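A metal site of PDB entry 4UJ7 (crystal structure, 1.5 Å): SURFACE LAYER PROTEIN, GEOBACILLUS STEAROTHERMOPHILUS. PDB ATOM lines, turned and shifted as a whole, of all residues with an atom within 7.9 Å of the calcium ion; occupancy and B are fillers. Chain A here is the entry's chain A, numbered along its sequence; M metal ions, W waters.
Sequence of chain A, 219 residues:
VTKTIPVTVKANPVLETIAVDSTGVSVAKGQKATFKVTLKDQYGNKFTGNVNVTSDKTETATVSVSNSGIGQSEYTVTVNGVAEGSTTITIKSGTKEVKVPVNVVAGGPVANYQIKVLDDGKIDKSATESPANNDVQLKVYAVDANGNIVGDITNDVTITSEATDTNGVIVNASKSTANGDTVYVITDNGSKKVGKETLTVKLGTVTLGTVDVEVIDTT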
ATOM      1  N   VAL A 117      12.808  -0.629   8.127  1.00  0.00           N
ATOM      2  CA  VAL A 117      14.002   0.110   7.670  1.00  0.00           C
ATOM      3  C   VAL A 117      15.023   0.093   8.789  1.00  0.00           C
ATOM      4  O   VAL A 117      14.767   0.646   9.883  1.00  0.00           O
ATOM      5  CB  VAL A 117      13.646   1.571   7.302  1.00  0.00           C
ATOM      6  CG1 VAL A 117      14.888   2.372   6.895  1.00  0.00           C
ATOM      7  CG2 VAL A 117      12.581   1.603   6.227  1.00  0.00           C
ATOM      8  N   LEU A 118      16.173  -0.542   8.548  1.00  0.00           N
ATOM      9  CA  LEU A 118      17.182  -0.728   9.601  1.00  0.00           C
ATOM     10  C   LEU A 118      18.083   0.480   9.812  1.00  0.00           C
ATOM     11  O   LEU A 118      18.553   0.730  10.924  1.00  0.00           O
ATOM     12  CB  LEU A 118      18.013  -1.976   9.311  1.00  0.00           C
ATOM     13  CG  LEU A 118      17.296  -3.331   9.309  1.00  0.00           C
ATOM     14  CD1 LEU A 118      18.258  -4.402   8.804  1.00  0.00           C
ATOM     15  CD2 LEU A 118      16.735  -3.689  10.676  1.00  0.00           C
ATOM     16  N   ASP A 119      18.329   1.223   8.735  1.00  0.00           N
ATOM     17  CA  ASP A 119      19.195   2.402   8.771  1.00  0.00           C
ATOM     18  C   ASP A 119      18.348   3.670   8.825  1.00  0.00           C
ATOM     19  O   ASP A 119      17.265   3.676   9.421  1.00  0.00           O
ATOM     20  CB  ASP A 119      20.156   2.395   7.576  1.00  0.00           C
ATOM     21  CG  ASP A 119      19.420   2.531   6.261  1.00  0.00           C
ATOM     22  OD1 ASP A 119      18.401   1.814   6.065  1.00  0.00           O
ATOM     23  OD2 ASP A 119      19.853   3.381   5.472  1.00  0.00           O
ATOM     24  N   ASP A 120      18.832   4.754   8.223  1.00  0.00           N
ATOM     25  CA  ASP A 120      18.079   6.018   8.152  1.00  0.00           C
ATOM     26  C   ASP A 120      17.054   6.113   7.020  1.00  0.00           C
ATOM     27  O   ASP A 120      16.304   7.076   6.953  1.00  0.00           O
ATOM     28  CB  ASP A 120      19.025   7.228   8.118  1.00  0.00           C
ATOM     29  CG  ASP A 120      19.817   7.343   6.816  1.00  0.00           C
ATOM     30  OD1 ASP A 120      19.774   6.409   5.989  1.00  0.00           O
ATOM     31  OD2 ASP A 120      20.486   8.386   6.644  1.00  0.00           O
ATOM     32  N   GLY A 121      17.020   5.112   6.137  1.00  0.00           N
ATOM     33  CA  GLY A 121      16.088   5.151   4.999  1.00  0.00           C
ATOM     34  C   GLY A 121      16.511   6.070   3.863  1.00  0.00           C
ATOM     35  O   GLY A 121      15.737   6.331   2.937  1.00  0.00           O
ATOM     36  N   LYS A 122      17.747   6.560   3.943  1.00  0.00           N
ATOM     37  CA  LYS A 122      18.287   7.516   2.989  1.00  0.00           C
ATOM     38  C   LYS A 122      19.551   6.993   2.311  1.00  0.00           C
ATOM     39  O   LYS A 122      20.335   6.252   2.919  1.00  0.00           O
ATOM     40  CB  LYS A 122      18.627   8.831   3.708  1.00  0.00           C
ATOM     41  CG  LYS A 122      17.461   9.410   4.488  1.00  0.00           C
ATOM     42  CD  LYS A 122      17.879  10.651   5.262  1.00  0.00           C
ATOM     43  CE  LYS A 122      16.732  11.114   6.145  1.00  0.00           C
ATOM     44  NZ  LYS A 122      15.431  10.939   5.446  1.00  0.00           N
ATOM     45  N   ILE A 123      19.728   7.398   1.046  1.00  0.00           N
ATOM     46  CA  ILE A 123      20.948   7.172   0.273  1.00  0.00           C
ATOM     47  C   ILE A 123      21.443   8.550  -0.161  1.00  0.00           C
ATOM     48  O   ILE A 123      20.711   9.319  -0.792  1.00  0.00           O
ATOM     49  CB  ILE A 123      20.663   6.315  -0.987  1.00  0.00           C
ATOM     50  CG1 ILE A 123      20.232   4.890  -0.600  1.00  0.00           C
ATOM     51  CG2 ILE A 123      21.865   6.319  -1.931  1.00  0.00           C
ATOM     52  CD1 ILE A 123      19.544   4.119  -1.711  1.00  0.00           C
ATOM     53  N   ASP A 124      22.690   8.872   0.199  1.00  0.00           N
ATOM     54  CA  ASP A 124      23.243  10.203  -0.056  1.00  0.00           C
ATOM     55  C   ASP A 124      24.123  10.150  -1.306  1.00  0.00           C
ATOM     56  O   ASP A 124      25.235   9.594  -1.254  1.00  0.00           O
ATOM     57  CB  ASP A 124      24.039  10.662   1.174  1.00  0.00           C
ATOM     58  CG  ASP A 124      24.437  12.136   1.120  1.00  0.00           C
ATOM     59  OD1 ASP A 124      24.399  12.754   0.036  1.00  0.00           O
ATOM     60  OD2 ASP A 124      24.796  12.656   2.200  1.00  0.00           O
ATOM     61  N   ALA A 132      29.982   7.763   5.413  1.00  0.00           N
ATOM     62  CA  ALA A 132      29.381   7.331   4.147  1.00  0.00           C
ATOM     63  C   ALA A 132      27.947   6.831   4.386  1.00  0.00           C
ATOM     64  O   ALA A 132      27.687   6.150   5.375  1.00  0.00           O
ATOM     65  CB  ALA A 132      30.224   6.253   3.499  1.00  0.00           C
ATOM     66  N   ASN A 133      27.036   7.182   3.490  1.00  0.00           N
ATOM     67  CA  ASN A 133      25.628   6.862   3.667  1.00  0.00           C
ATOM     68  C   ASN A 133      25.041   6.436   2.327  1.00  0.00           C
ATOM     69  O   ASN A 133      24.223   7.137   1.720  1.00  0.00           O
ATOM     70  CB  ASN A 133      24.886   8.091   4.212  1.00  0.00           C
ATOM     71  CG  ASN A 133      23.435   7.805   4.581  1.00  0.00           C
ATOM     72  OD1 ASN A 133      23.004   6.643   4.613  1.00  0.00           O
ATOM     73  ND2 ASN A 133      22.680   8.867   4.826  1.00  0.00           N
ATOM     74  N   ASN A 134      25.472   5.263   1.871  1.00  0.00           N
ATOM     75  CA  ASN A 134      25.231   4.880   0.478  1.00  0.00           C
ATOM     76  C   ASN A 134      24.250   3.744   0.279  1.00  0.00           C
ATOM     77  O   ASN A 134      24.114   3.195  -0.824  1.00  0.00           O
ATOM     78  CB  ASN A 134      26.572   4.598  -0.204  1.00  0.00           C
ATOM     79  CG  ASN A 134      27.413   5.862  -0.371  1.00  0.00           C
ATOM     80  OD1 ASN A 134      26.907   6.924  -0.760  1.00  0.00           O
ATOM     81  ND2 ASN A 134      28.703   5.732  -0.086  1.00  0.00           N
ATOM     82  N   ASP A 135      23.527   3.386   1.323  1.00  0.00           N
ATOM     83  CA  ASP A 135      22.504   2.364   1.167  1.00  0.00           C
ATOM     84  C   ASP A 135      21.290   2.569   2.047  1.00  0.00           C
ATOM     85  O   ASP A 135      21.256   3.475   2.898  1.00  0.00           O
ATOM     86  CB  ASP A 135      23.097   0.937   1.289  1.00  0.00           C
ATOM     87  CG  ASP A 135      23.428   0.507   2.728  1.00  0.00           C
ATOM     88  OD1 ASP A 135      22.972   1.127   3.713  1.00  0.00           O
ATOM     89  OD2 ASP A 135      24.118  -0.519   2.863  1.00  0.00           O
ATOM     90  N   VAL A 136      20.275   1.740   1.782  1.00  0.00           N
ATOM     91  CA  VAL A 136      19.191   1.492   2.723  1.00  0.00           C
ATOM     92  C   VAL A 136      19.194  -0.013   2.947  1.00  0.00           C
ATOM     93  O   VAL A 136      19.498  -0.776   2.034  1.00  0.00           O
ATOM     94  CB  VAL A 136      17.825   1.969   2.184  1.00  0.00           C
ATOM     95  CG1 VAL A 136      16.674   1.511   3.071  1.00  0.00           C
ATOM     96  CG2 VAL A 136      17.837   3.489   2.044  1.00  0.00           C
ATOM     97  N   GLN A 137      18.881  -0.417   4.167  1.00  0.00           N
ATOM     98  CA  GLN A 137      18.799  -1.823   4.508  1.00  0.00           C
ATOM     99  C   GLN A 137      17.406  -2.150   5.023  1.00  0.00           C
ATOM    100  O   GLN A 137      16.895  -1.471   5.918  1.00  0.00           O
ATOM    101  CB  GLN A 137      19.799  -2.143   5.610  1.00  0.00           C
ATOM    102  CG  GLN A 137      21.227  -2.253   5.103  1.00  0.00           C
ATOM    103  CD  GLN A 137      22.108  -2.808   6.195  1.00  0.00           C
ATOM    104  OE1 GLN A 137      22.198  -2.239   7.288  1.00  0.00           O
ATOM    105  NE2 GLN A 137      22.725  -3.933   5.921  1.00  0.00           N
ATOM    106  N   ILE A 186      19.533  -1.647  -0.646  1.00  0.00           N
ATOM    107  CA  ILE A 186      19.142  -0.692  -1.694  1.00  0.00           C
ATOM    108  C   ILE A 186      20.299   0.283  -1.920  1.00  0.00           C
ATOM    109  O   ILE A 186      20.819   0.878  -0.966  1.00  0.00           O
ATOM    110  CB  ILE A 186      17.879   0.099  -1.259  1.00  0.00           C
ATOM    111  CG1 ILE A 186      16.812  -0.804  -0.589  1.00  0.00           C
ATOM    112  CG2 ILE A 186      17.308   0.850  -2.461  1.00  0.00           C
ATOM    113  CD1 ILE A 186      16.367  -1.978  -1.456  1.00  0.00           C
ATOM    114  N   GLU A 214      14.575   7.269   0.221  1.00  0.00           N
ATOM    115  CA  GLU A 214      14.858   8.649  -0.188  1.00  0.00           C
ATOM    116  C   GLU A 214      16.300   8.807  -0.631  1.00  0.00           C
ATOM    117  O   GLU A 214      17.221   8.431   0.101  1.00  0.00           O
ATOM    118  CB  GLU A 214      14.557   9.620   0.967  1.00  0.00           C
ATOM    119  CG  GLU A 214      14.601  11.091   0.560  1.00  0.00           C
ATOM    120  CD  GLU A 214      14.402  12.059   1.721  1.00  0.00           C
ATOM    121  OE1 GLU A 214      14.138  11.599   2.856  1.00  0.00           O
ATOM    122  OE2 GLU A 214      14.505  13.293   1.498  1.00  0.00           O
ATOM    123  N   ILE A 216      19.037  11.564  -1.146  1.00  0.00           N
ATOM    124  CA  ILE A 216      19.396  12.937  -0.755  1.00  0.00           C
ATOM    125  C   ILE A 216      20.761  13.274  -1.378  1.00  0.00           C
ATOM    126  O   ILE A 216      21.447  12.402  -1.941  1.00  0.00           O
ATOM    127  CB  ILE A 216      19.422  13.109   0.801  1.00  0.00           C
ATOM    128  CG1 ILE A 216      20.557  12.274   1.430  1.00  0.00           C
ATOM    129  CG2 ILE A 216      18.056  12.802   1.394  1.00  0.00           C
ATOM    130  CD1 ILE A 216      20.827  12.545   2.920  1.00  0.00           C
HETATM  131 CA    CA M   1      21.376   5.040   4.730  1.00  0.00          CA
HETATM  132  O   HOH W   1      22.196   5.019   7.042  1.00  0.00           O
HETATM  133  O   HOH W   2      23.552   3.674   4.510  1.00  0.00           O
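Five residues have an atom within 4 Å of the calcium ion: Asp 119, Asp 120, Lys 122, Asn 133 and Asp 135.
The calcium ion is bound by OD1 of Asn 133, OD2 of Asp 119, O of Asp 135, O of Lys 122, water W1, OD1 of Asp 120 and water W2.
The calcium ion has seven donor atoms within binding distance.
The side-chain carboxylate (OD1) of Asp 119 lies within hydrogen-bond range of the backbone NH (N) of Gln 137 (3.0 Å).
NZ of Lys 122 is in salt-bridge range of OE1 of Glu 214, 3.0 Å away.
The backbone carbonyl oxygen (O) of Asn 133 lies within hydrogen-bond range of the backbone NH (N) of Asp 124, 2.8 Å away.
The side-chain carboxylate (OD2) of Asp 119 sits close to the backbone NH (N) of Gly 121 (3.4 Å).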
